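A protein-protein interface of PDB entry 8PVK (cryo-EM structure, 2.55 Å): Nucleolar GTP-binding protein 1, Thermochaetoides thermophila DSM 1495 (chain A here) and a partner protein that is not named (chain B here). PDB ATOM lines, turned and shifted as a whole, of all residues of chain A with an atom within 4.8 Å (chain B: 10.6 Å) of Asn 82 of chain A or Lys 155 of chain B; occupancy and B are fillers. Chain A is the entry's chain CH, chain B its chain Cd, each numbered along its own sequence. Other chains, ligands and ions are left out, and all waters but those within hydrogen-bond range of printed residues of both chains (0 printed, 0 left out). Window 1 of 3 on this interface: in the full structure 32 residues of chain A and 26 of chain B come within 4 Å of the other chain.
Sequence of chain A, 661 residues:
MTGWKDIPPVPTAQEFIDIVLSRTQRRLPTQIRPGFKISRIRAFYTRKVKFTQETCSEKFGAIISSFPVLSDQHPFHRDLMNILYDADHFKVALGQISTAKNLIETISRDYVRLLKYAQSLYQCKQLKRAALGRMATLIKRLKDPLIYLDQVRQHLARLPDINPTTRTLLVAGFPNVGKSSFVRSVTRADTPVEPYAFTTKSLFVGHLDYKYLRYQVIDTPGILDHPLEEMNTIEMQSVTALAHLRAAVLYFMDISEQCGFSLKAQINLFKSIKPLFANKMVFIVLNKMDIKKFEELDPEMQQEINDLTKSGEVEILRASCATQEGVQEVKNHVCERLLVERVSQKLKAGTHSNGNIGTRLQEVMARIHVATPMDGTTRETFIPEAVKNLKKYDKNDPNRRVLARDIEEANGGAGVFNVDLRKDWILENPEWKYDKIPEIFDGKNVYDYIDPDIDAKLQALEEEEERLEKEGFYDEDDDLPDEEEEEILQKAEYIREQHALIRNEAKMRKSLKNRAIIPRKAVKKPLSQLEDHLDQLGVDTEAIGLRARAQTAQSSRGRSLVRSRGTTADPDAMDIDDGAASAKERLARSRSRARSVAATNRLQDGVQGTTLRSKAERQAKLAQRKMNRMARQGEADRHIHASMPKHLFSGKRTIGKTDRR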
ATOM      1  N   ARG A  78       7.617  -7.249   6.552  1.00  0.00           N
ATOM      2  CA  ARG A  78       8.108  -7.499   5.199  1.00  0.00           C
ATOM      3  C   ARG A  78       6.956  -7.706   4.222  1.00  0.00           C
ATOM      4  O   ARG A  78       6.922  -7.102   3.141  1.00  0.00           O
ATOM      5  CB  ARG A  78       9.033  -8.716   5.210  1.00  0.00           C
ATOM      6  CG  ARG A  78       9.471  -9.198   3.840  1.00  0.00           C
ATOM      7  CD  ARG A  78      10.435 -10.367   3.961  1.00  0.00           C
ATOM      8  NE  ARG A  78      11.179 -10.332   5.215  1.00  0.00           N
ATOM      9  CZ  ARG A  78      11.339 -11.373   6.021  1.00  0.00           C
ATOM     10  NH1 ARG A  78      10.819 -12.555   5.737  1.00  0.00           N
ATOM     11  NH2 ARG A  78      12.038 -11.223   7.144  1.00  0.00           N
ATOM     12  N   ASP A  79       5.975  -8.525   4.603  1.00  0.00           N
ATOM     13  CA  ASP A  79       4.851  -8.769   3.709  1.00  0.00           C
ATOM     14  C   ASP A  79       3.911  -7.572   3.641  1.00  0.00           C
ATOM     15  O   ASP A  79       3.293  -7.339   2.598  1.00  0.00           O
ATOM     16  CB  ASP A  79       4.108 -10.030   4.138  1.00  0.00           C
ATOM     17  CG  ASP A  79       4.816 -11.292   3.692  1.00  0.00           C
ATOM     18  OD1 ASP A  79       5.256 -11.342   2.524  1.00  0.00           O
ATOM     19  OD2 ASP A  79       4.953 -12.225   4.507  1.00  0.00           O
ATOM     20  N   LEU A  80       3.815  -6.782   4.715  1.00  0.00           N
ATOM     21  CA  LEU A  80       3.023  -5.558   4.669  1.00  0.00           C
ATOM     22  C   LEU A  80       3.638  -4.539   3.722  1.00  0.00           C
ATOM     23  O   LEU A  80       2.921  -3.879   2.963  1.00  0.00           O
ATOM     24  CB  LEU A  80       2.891  -4.968   6.071  1.00  0.00           C
ATOM     25  CG  LEU A  80       2.026  -3.713   6.191  1.00  0.00           C
ATOM     26  CD1 LEU A  80       0.587  -4.010   5.804  1.00  0.00           C
ATOM     27  CD2 LEU A  80       2.111  -3.132   7.589  1.00  0.00           C
ATOM     28  N   MET A  81       4.965  -4.393   3.755  1.00  0.00           N
ATOM     29  CA  MET A  81       5.634  -3.500   2.816  1.00  0.00           C
ATOM     30  C   MET A  81       5.544  -4.025   1.391  1.00  0.00           C
ATOM     31  O   MET A  81       5.478  -3.230   0.445  1.00  0.00           O
ATOM     32  CB  MET A  81       7.090  -3.299   3.232  1.00  0.00           C
ATOM     33  CG  MET A  81       7.240  -2.535   4.538  1.00  0.00           C
ATOM     34  SD  MET A  81       8.941  -2.285   5.074  1.00  0.00           S
ATOM     35  CE  MET A  81       8.665  -1.469   6.642  1.00  0.00           C
ATOM     36  N   ASN A  82       5.531  -5.351   1.217  1.00  0.00           N
ATOM     37  CA  ASN A  82       5.281  -5.923  -0.103  1.00  0.00           C
ATOM     38  C   ASN A  82       3.882  -5.581  -0.605  1.00  0.00           C
ATOM     39  O   ASN A  82       3.701  -5.262  -1.785  1.00  0.00           O
ATOM     40  CB  ASN A  82       5.474  -7.439  -0.066  1.00  0.00           C
ATOM     41  CG  ASN A  82       4.963  -8.122  -1.320  1.00  0.00           C
ATOM     42  OD1 ASN A  82       5.418  -7.835  -2.426  1.00  0.00           O
ATOM     43  ND2 ASN A  82       4.009  -9.030  -1.153  1.00  0.00           N
ATOM     44  N   ILE A  83       2.880  -5.659   0.274  1.00  0.00           N
ATOM     45  CA  ILE A  83       1.510  -5.330  -0.115  1.00  0.00           C
ATOM     46  C   ILE A  83       1.382  -3.845  -0.442  1.00  0.00           C
ATOM     47  O   ILE A  83       0.777  -3.467  -1.453  1.00  0.00           O
ATOM     48  CB  ILE A  83       0.523  -5.752   0.993  1.00  0.00           C
ATOM     49  CG1 ILE A  83       0.460  -7.274   1.117  1.00  0.00           C
ATOM     50  CG2 ILE A  83      -0.869  -5.192   0.735  1.00  0.00           C
ATOM     51  CD1 ILE A  83       0.000  -7.973  -0.127  1.00  0.00           C
ATOM     52  N   LEU A  84       1.962  -2.983   0.393  1.00  0.00           N
ATOM     53  CA  LEU A  84       1.765  -1.547   0.240  1.00  0.00           C
ATOM     54  C   LEU A  84       2.577  -0.962  -0.911  1.00  0.00           C
ATOM     55  O   LEU A  84       2.070  -0.115  -1.656  1.00  0.00           O
ATOM     56  CB  LEU A  84       2.115  -0.826   1.543  1.00  0.00           C
ATOM     57  CG  LEU A  84       1.185  -1.055   2.735  1.00  0.00           C
ATOM     58  CD1 LEU A  84       1.715  -0.347   3.970  1.00  0.00           C
ATOM     59  CD2 LEU A  84      -0.225  -0.595   2.412  1.00  0.00           C
ATOM     60  N   TYR A  85       3.831  -1.386  -1.080  1.00  0.00           N
ATOM     61  CA  TYR A  85       4.749  -0.674  -1.959  1.00  0.00           C
ATOM     62  C   TYR A  85       5.330  -1.518  -3.085  1.00  0.00           C
ATOM     63  O   TYR A  85       6.171  -1.001  -3.829  1.00  0.00           O
ATOM     64  CB  TYR A  85       5.903  -0.069  -1.152  1.00  0.00           C
ATOM     65  CG  TYR A  85       5.487   0.622   0.121  1.00  0.00           C
ATOM     66  CD1 TYR A  85       4.605   1.692   0.094  1.00  0.00           C
ATOM     67  CD2 TYR A  85       5.991   0.216   1.349  1.00  0.00           C
ATOM     68  CE1 TYR A  85       4.229   2.332   1.254  1.00  0.00           C
ATOM     69  CE2 TYR A  85       5.619   0.849   2.515  1.00  0.00           C
ATOM     70  CZ  TYR A  85       4.737   1.906   2.462  1.00  0.00           C
ATOM     71  OH  TYR A  85       4.365   2.539   3.623  1.00  0.00           O
ATOM     72  N   ASP A  86       4.914  -2.784  -3.232  1.00  0.00           N
ATOM     73  CA  ASP A  86       5.441  -3.686  -4.260  1.00  0.00           C
ATOM     74  C   ASP A  86       6.951  -3.865  -4.128  1.00  0.00           C
ATOM     75  O   ASP A  86       7.731  -3.192  -4.819  1.00  0.00           O
ATOM     76  CB  ASP A  86       5.065  -3.234  -5.674  1.00  0.00           C
ATOM     77  CG  ASP A  86       5.322  -4.305  -6.713  1.00  0.00           C
ATOM     78  OD1 ASP A  86       5.424  -5.492  -6.335  1.00  0.00           O
ATOM     79  OD2 ASP A  86       5.415  -3.967  -7.909  1.00  0.00           O
ATOM     80  N   ALA A  87       7.352  -4.689  -3.153  1.00  0.00           N
ATOM     81  CA  ALA A  87       8.730  -5.029  -2.798  1.00  0.00           C
ATOM     82  C   ALA A  87       9.696  -5.165  -3.973  1.00  0.00           C
ATOM     83  O   ALA A  87      10.860  -4.771  -3.858  1.00  0.00           O
ATOM     84  CB  ALA A  87       8.736  -6.334  -1.998  1.00  0.00           C
ATOM     85  N   ASP A  88       9.229  -5.715  -5.099  1.00  0.00           N
ATOM     86  CA  ASP A  88      10.043  -5.747  -6.312  1.00  0.00           C
ATOM     87  C   ASP A  88      10.416  -4.340  -6.770  1.00  0.00           C
ATOM     88  O   ASP A  88      11.595  -4.043  -6.990  1.00  0.00           O
ATOM     89  CB  ASP A  88       9.300  -6.491  -7.421  1.00  0.00           C
ATOM     90  CG  ASP A  88       9.617  -7.970  -7.445  1.00  0.00           C
ATOM     91  OD1 ASP A  88      10.707  -8.353  -6.973  1.00  0.00           O
ATOM     92  OD2 ASP A  88       8.777  -8.750  -7.938  1.00  0.00           O
ATOM     93  N   GLN B 131      15.784  -8.809 -15.241  1.00  0.00           N
ATOM     94  CA  GLN B 131      14.557  -8.877 -14.445  1.00  0.00           C
ATOM     95  C   GLN B 131      14.075  -7.500 -13.994  1.00  0.00           C
ATOM     96  O   GLN B 131      12.873  -7.214 -14.047  1.00  0.00           O
ATOM     97  CB  GLN B 131      14.762  -9.777 -13.226  1.00  0.00           C
ATOM     98  CG  GLN B 131      14.461 -11.242 -13.466  1.00  0.00           C
ATOM     99  CD  GLN B 131      13.088 -11.461 -14.064  1.00  0.00           C
ATOM    100  OE1 GLN B 131      12.959 -11.837 -15.229  1.00  0.00           O
ATOM    101  NE2 GLN B 131      12.052 -11.225 -13.269  1.00  0.00           N
ATOM    102  N   MET B 134      12.751  -5.538 -16.894  1.00  0.00           N
ATOM    103  CA  MET B 134      11.523  -6.179 -17.344  1.00  0.00           C
ATOM    104  C   MET B 134      10.347  -5.821 -16.442  1.00  0.00           C
ATOM    105  O   MET B 134       9.244  -5.551 -16.931  1.00  0.00           O
ATOM    106  CB  MET B 134      11.742  -7.688 -17.386  1.00  0.00           C
ATOM    107  CG  MET B 134      10.614  -8.509 -17.951  1.00  0.00           C
ATOM    108  SD  MET B 134      11.115 -10.235 -17.903  1.00  0.00           S
ATOM    109  CE  MET B 134      12.351 -10.231 -19.201  1.00  0.00           C
ATOM    110  N   THR B 135      10.568  -5.798 -15.124  1.00  0.00           N
ATOM    111  CA  THR B 135       9.503  -5.414 -14.201  1.00  0.00           C
ATOM    112  C   THR B 135       9.140  -3.942 -14.350  1.00  0.00           C
ATOM    113  O   THR B 135       7.962  -3.579 -14.248  1.00  0.00           O
ATOM    114  CB  THR B 135       9.902  -5.717 -12.756  1.00  0.00           C
ATOM    115  OG1 THR B 135      11.155  -5.090 -12.458  1.00  0.00           O
ATOM    116  CG2 THR B 135      10.004  -7.217 -12.528  1.00  0.00           C
ATOM    117  N   ARG B 138       7.089  -3.679 -17.465  1.00  0.00           N
ATOM    118  CA  ARG B 138       5.750  -4.218 -17.249  1.00  0.00           C
ATOM    119  C   ARG B 138       4.886  -3.249 -16.449  1.00  0.00           C
ATOM    120  O   ARG B 138       3.745  -2.962 -16.828  1.00  0.00           O
ATOM    121  CB  ARG B 138       5.848  -5.569 -16.544  1.00  0.00           C
ATOM    122  CG  ARG B 138       4.535  -6.314 -16.412  1.00  0.00           C
ATOM    123  CD  ARG B 138       4.659  -7.486 -15.448  1.00  0.00           C
ATOM    124  NE  ARG B 138       5.891  -8.240 -15.644  1.00  0.00           N
ATOM    125  CZ  ARG B 138       6.849  -8.360 -14.735  1.00  0.00           C
ATOM    126  NH1 ARG B 138       6.750  -7.788 -13.546  1.00  0.00           N
ATOM    127  NH2 ARG B 138       7.934  -9.071 -15.026  1.00  0.00           N
ATOM    128  N   GLU B 139       5.411  -2.735 -15.342  1.00  0.00           N
ATOM    129  CA  GLU B 139       4.710  -1.748 -14.523  1.00  0.00           C
ATOM    130  C   GLU B 139       5.652  -0.594 -14.218  1.00  0.00           C
ATOM    131  O   GLU B 139       6.653  -0.792 -13.499  1.00  0.00           O
ATOM    132  CB  GLU B 139       4.189  -2.363 -13.226  1.00  0.00           C
ATOM    133  CG  GLU B 139       3.085  -3.388 -13.405  1.00  0.00           C
ATOM    134  CD  GLU B 139       3.565  -4.807 -13.186  1.00  0.00           C
ATOM    135  OE1 GLU B 139       4.738  -4.989 -12.800  1.00  0.00           O
ATOM    136  OE2 GLU B 139       2.762  -5.741 -13.391  1.00  0.00           O
ATOM    137  N   THR B 144       2.462   2.130  -9.960  1.00  0.00           N
ATOM    138  CA  THR B 144       2.570   1.237  -8.813  1.00  0.00           C
ATOM    139  C   THR B 144       2.210   1.924  -7.503  1.00  0.00           C
ATOM    140  O   THR B 144       1.328   1.455  -6.778  1.00  0.00           O
ATOM    141  CB  THR B 144       3.990   0.667  -8.731  1.00  0.00           C
ATOM    142  OG1 THR B 144       4.289  -0.047  -9.935  1.00  0.00           O
ATOM    143  CG2 THR B 144       4.111  -0.267  -7.552  1.00  0.00           C
ATOM    144  N   PHE B 145       2.875   3.030  -7.184  1.00  0.00           N
ATOM    145  CA  PHE B 145       2.580   3.794  -5.983  1.00  0.00           C
ATOM    146  C   PHE B 145       2.598   5.275  -6.327  1.00  0.00           C
ATOM    147  O   PHE B 145       3.345   5.713  -7.205  1.00  0.00           O
ATOM    148  CB  PHE B 145       3.581   3.493  -4.860  1.00  0.00           C
ATOM    149  CG  PHE B 145       3.085   3.861  -3.492  1.00  0.00           C
ATOM    150  CD1 PHE B 145       2.168   3.059  -2.834  1.00  0.00           C
ATOM    151  CD2 PHE B 145       3.535   5.010  -2.864  1.00  0.00           C
ATOM    152  CE1 PHE B 145       1.708   3.398  -1.576  1.00  0.00           C
ATOM    153  CE2 PHE B 145       3.082   5.353  -1.607  1.00  0.00           C
ATOM    154  CZ  PHE B 145       2.167   4.546  -0.962  1.00  0.00           C
ATOM    155  N   ARG B 151      -2.308   0.245  -9.437  1.00  0.00           N
ATOM    156  CA  ARG B 151      -2.056  -1.109  -8.966  1.00  0.00           C
ATOM    157  C   ARG B 151      -3.118  -1.502  -7.945  1.00  0.00           C
ATOM    158  O   ARG B 151      -3.270  -0.845  -6.911  1.00  0.00           O
ATOM    159  CB  ARG B 151      -0.656  -1.202  -8.364  1.00  0.00           C
ATOM    160  CG  ARG B 151      -0.408  -2.431  -7.509  1.00  0.00           C
ATOM    161  CD  ARG B 151       1.030  -2.459  -7.022  1.00  0.00           C
ATOM    162  NE  ARG B 151       1.259  -3.495  -6.020  1.00  0.00           N
ATOM    163  CZ  ARG B 151       1.267  -3.280  -4.712  1.00  0.00           C
ATOM    164  NH1 ARG B 151       1.047  -2.077  -4.207  1.00  0.00           N
ATOM    165  NH2 ARG B 151       1.500  -4.298  -3.889  1.00  0.00           N
ATOM    166  N   LYS B 152      -3.851  -2.572  -8.239  1.00  0.00           N
ATOM    167  CA  LYS B 152      -4.886  -3.082  -7.353  1.00  0.00           C
ATOM    168  C   LYS B 152      -4.596  -4.471  -6.811  1.00  0.00           C
ATOM    169  O   LYS B 152      -4.949  -4.756  -5.666  1.00  0.00           O
ATOM    170  CB  LYS B 152      -6.243  -3.109  -8.073  1.00  0.00           C
ATOM    171  CG  LYS B 152      -6.943  -1.763  -8.139  1.00  0.00           C
ATOM    172  CD  LYS B 152      -7.466  -1.351  -6.776  1.00  0.00           C
ATOM    173  CE  LYS B 152      -8.223  -0.038  -6.850  1.00  0.00           C
ATOM    174  NZ  LYS B 152      -8.644   0.425  -5.502  1.00  0.00           N
ATOM    175  N   ARG B 153      -3.963  -5.341  -7.598  1.00  0.00           N
ATOM    176  CA  ARG B 153      -3.674  -6.707  -7.190  1.00  0.00           C
ATOM    177  C   ARG B 153      -2.200  -6.838  -6.848  1.00  0.00           C
ATOM    178  O   ARG B 153      -1.349  -6.551  -7.703  1.00  0.00           O
ATOM    179  CB  ARG B 153      -4.050  -7.685  -8.302  1.00  0.00           C
ATOM    180  CG  ARG B 153      -5.511  -7.635  -8.702  1.00  0.00           C
ATOM    181  CD  ARG B 153      -6.402  -8.201  -7.615  1.00  0.00           C
ATOM    182  NE  ARG B 153      -7.811  -8.133  -7.984  1.00  0.00           N
ATOM    183  CZ  ARG B 153      -8.450  -9.068  -8.672  1.00  0.00           C
ATOM    184  NH1 ARG B 153      -7.829 -10.153  -9.106  1.00  0.00           N
ATOM    185  NH2 ARG B 153      -9.743  -8.909  -8.937  1.00  0.00           N
ATOM    186  N   PRO B 154      -1.846  -7.254  -5.638  1.00  0.00           N
ATOM    187  CA  PRO B 154      -0.434  -7.422  -5.293  1.00  0.00           C
ATOM    188  C   PRO B 154       0.130  -8.715  -5.868  1.00  0.00           C
ATOM    189  O   PRO B 154      -0.593  -9.598  -6.331  1.00  0.00           O
ATOM    190  CB  PRO B 154      -0.453  -7.457  -3.763  1.00  0.00           C
ATOM    191  CG  PRO B 154      -1.785  -8.033  -3.432  1.00  0.00           C
ATOM    192  CD  PRO B 154      -2.737  -7.589  -4.514  1.00  0.00           C
ATOM    193  N   LYS B 155       1.456  -8.810  -5.831  1.00  0.00           N
ATOM    194  CA  LYS B 155       2.174  -9.992  -6.288  1.00  0.00           C
ATOM    195  C   LYS B 155       2.523 -10.845  -5.076  1.00  0.00           C
ATOM    196  O   LYS B 155       3.240 -10.390  -4.178  1.00  0.00           O
ATOM    197  CB  LYS B 155       3.434  -9.600  -7.059  1.00  0.00           C
ATOM    198  CG  LYS B 155       4.208 -10.776  -7.628  1.00  0.00           C
ATOM    199  CD  LYS B 155       5.479 -10.310  -8.319  1.00  0.00           C
ATOM    200  CE  LYS B 155       6.354 -11.485  -8.722  1.00  0.00           C
ATOM    201  NZ  LYS B 155       6.772 -12.296  -7.547  1.00  0.00           N
ATOM    202  N   LEU B 156       2.020 -12.075  -5.054  1.00  0.00           N
ATOM    203  CA  LEU B 156       2.144 -12.950  -3.901  1.00  0.00           C
ATOM    204  C   LEU B 156       2.913 -14.210  -4.272  1.00  0.00           C
ATOM    205  O   LEU B 156       2.854 -14.684  -5.409  1.00  0.00           O
ATOM    206  CB  LEU B 156       0.768 -13.333  -3.347  1.00  0.00           C
ATOM    207  CG  LEU B 156      -0.174 -12.178  -3.004  1.00  0.00           C
ATOM    208  CD1 LEU B 156      -1.535 -12.709  -2.594  1.00  0.00           C
ATOM    209  CD2 LEU B 156       0.418 -11.307  -1.912  1.00  0.00           C
ATOM    210  N   SER B 157       3.635 -14.748  -3.292  1.00  0.00           N
ATOM    211  CA  SER B 157       4.365 -15.998  -3.443  1.00  0.00           C
ATOM    212  C   SER B 157       3.531 -17.208  -3.046  1.00  0.00           C
ATOM    213  O   SER B 157       4.054 -18.327  -3.016  1.00  0.00           O
ATOM    214  CB  SER B 157       5.650 -15.959  -2.614  1.00  0.00           C
ATOM    215  OG  SER B 157       6.361 -17.179  -2.720  1.00  0.00           O
ATOM    216  N   PHE B 158       2.252 -17.006  -2.742  1.00  0.00           N
ATOM    217  CA  PHE B 158       1.360 -18.070  -2.309  1.00  0.00           C
ATOM    218  C   PHE B 158       0.046 -17.941  -3.062  1.00  0.00           C
ATOM    219  O   PHE B 158      -0.331 -16.858  -3.515  1.00  0.00           O
ATOM    220  CB  PHE B 158       1.120 -18.024  -0.792  1.00  0.00           C
ATOM    221  CG  PHE B 158       0.916 -16.634  -0.250  1.00  0.00           C
ATOM    222  CD1 PHE B 158      -0.345 -16.066  -0.221  1.00  0.00           C
ATOM    223  CD2 PHE B 158       1.986 -15.901   0.242  1.00  0.00           C
ATOM    224  CE1 PHE B 158      -0.535 -14.790   0.274  1.00  0.00           C
ATOM    225  CE2 PHE B 158       1.803 -14.627   0.738  1.00  0.00           C
ATOM    226  CZ  PHE B 158       0.541 -14.070   0.752  1.00  0.00           C
ATOM    227  N   ASN B 159      -0.651 -19.062  -3.195  1.00  0.00           N
ATOM    228  CA  ASN B 159      -1.909 -19.101  -3.930  1.00  0.00           C
ATOM    229  C   ASN B 159      -3.098 -19.367  -3.021  1.00  0.00           C
ATOM    230  O   ASN B 159      -4.142 -18.726  -3.173  1.00  0.00           O
ATOM    231  CB  ASN B 159      -1.822 -20.181  -5.031  1.00  0.00           C
ATOM    232  CG  ASN B 159      -3.000 -20.159  -6.008  1.00  0.00           C
ATOM    233  OD1 ASN B 159      -3.930 -19.361  -5.893  1.00  0.00           O
ATOM    234  ND2 ASN B 159      -2.954 -21.055  -6.985  1.00  0.00           N
ATOM    235  N   LEU B 164      -0.310 -20.089   2.355  1.00  0.00           N
ATOM    236  CA  LEU B 164       0.018 -18.893   3.126  1.00  0.00           C
ATOM    237  C   LEU B 164       0.408 -19.241   4.559  1.00  0.00           C
ATOM    238  O   LEU B 164       1.342 -18.652   5.111  1.00  0.00           O
ATOM    239  CB  LEU B 164      -1.164 -17.924   3.111  1.00  0.00           C
ATOM    240  CG  LEU B 164      -1.109 -16.686   4.010  1.00  0.00           C
ATOM    241  CD1 LEU B 164       0.154 -15.863   3.796  1.00  0.00           C
ATOM    242  CD2 LEU B 164      -2.339 -15.840   3.783  1.00  0.00           C
ATOM    243  N   TYR B 167       3.828 -20.839   4.428  1.00  0.00           N
ATOM    244  CA  TYR B 167       4.787 -19.795   4.092  1.00  0.00           C
ATOM    245  C   TYR B 167       5.069 -18.896   5.286  1.00  0.00           C
ATOM    246  O   TYR B 167       6.215 -18.500   5.507  1.00  0.00           O
ATOM    247  CB  TYR B 167       4.260 -18.978   2.913  1.00  0.00           C
ATOM    248  CG  TYR B 167       5.187 -17.884   2.444  1.00  0.00           C
ATOM    249  CD1 TYR B 167       6.317 -18.180   1.694  1.00  0.00           C
ATOM    250  CD2 TYR B 167       4.926 -16.552   2.740  1.00  0.00           C
ATOM    251  CE1 TYR B 167       7.166 -17.181   1.259  1.00  0.00           C
ATOM    252  CE2 TYR B 167       5.769 -15.546   2.310  1.00  0.00           C
ATOM    253  CZ  TYR B 167       6.887 -15.867   1.570  1.00  0.00           C
ATOM    254  OH  TYR B 167       7.730 -14.869   1.138  1.00  0.00           O
ATOM    255  N   SER B 171       8.589 -18.494   7.061  1.00  0.00           N
ATOM    256  CA  SER B 171       9.134 -17.144   7.150  1.00  0.00           C
ATOM    257  C   SER B 171       9.494 -16.780   8.583  1.00  0.00           C
ATOM    258  O   SER B 171      10.527 -16.147   8.823  1.00  0.00           O
ATOM    259  CB  SER B 171       8.134 -16.142   6.571  1.00  0.00           C
ATOM    260  OG  SER B 171       7.935 -16.362   5.186  1.00  0.00           O
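The backbone carbonyl oxygen of Lys 155 of chain B is in hydrogen-bond range of the side-chain amide nitrogen of Asn 82 of chain A, 3.4 Å away. O of Ile 83 of chain A sits at hydrogen-bond distance from NH2 of Arg 151 of chain B (2.7 Å). The guanidinium group (NH1) of Arg 151 of chain B is in hydrogen-bond range of the backbone carbonyl oxygen (O) of Leu 84 of chain A, 3.4 Å away. O of Asn 82 of chain A lies within hydrogen-bond range of NH2 of Arg 151 of chain B (3.2 Å).
Ile 83 of chain A touches Pro 154 of chain B. CD1 of Ile 83 of chain A touches CD2 of Leu 156 of chain B, 3.8 Å away. Leu 84 of chain A touches Phe 145 of chain B. Tyr 85 of chain A touches Phe 145 of chain B. Thr 144 of chain B touches Asp 86 of chain A (CG2 to CB, 3.6 Å). Asp 86 of chain A touches Arg 151 of chain B. Asp 88 of chain A touches Lys 155 of chain B.
Asn 82 of chain A touches two residues of chain B. Of chain A, only Asn 82 (3.4 Å) and Asp 88 (3.7 Å) come within 4 Å of Lys 155 of chain B. Ile 83 of chain A touches just these residues of chain B: Arg 151 (2.7 Å), Pro 154 (3.7 Å) and Leu 156 (3.8 Å). Of the printed residues of chain B, Asp 86 of chain A touches Thr 144 and Arg 151. Ala 87 of chain A touches none of the printed residues of chain B. Printed residues of chain A within 4 Å of Pro 154 of chain B: Ile 83 (3.7 Å). Printed residues of chain B within 4 Å of Leu 84 of chain A: Phe 145 (3.4 Å) and Arg 151 (3.4 Å). Printed residues of chain A within 4 Å of Leu 156 of chain B: Ile 83. Arg 138 of chain B touches none of the printed residues of chain A. The nearest residue of chain A that does not touch Lys 155 of chain B is Asp 86 of chain A (4.6 Å).
Printed residues of chain B that touch a printed residue of chain A: Thr 144, Phe 145, Arg 151, Pro 154, Lys 155 and Leu 156. Hydrophobic or aromatic side chains of chain B that line the printed part of chain A: Phe 145, Pro 154 and Leu 156. Of the 11 printed residues of chain A, 6 touch a printed residue of chain B. Hydrophobic or aromatic side chains of chain A within 4 Å of the printed part of chain B: Ile 83 and Tyr 85. Among the printed residues, no Asp or Glu carboxylate lies within 4 Å of a Lys or Arg side-chain nitrogen of the other chain.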
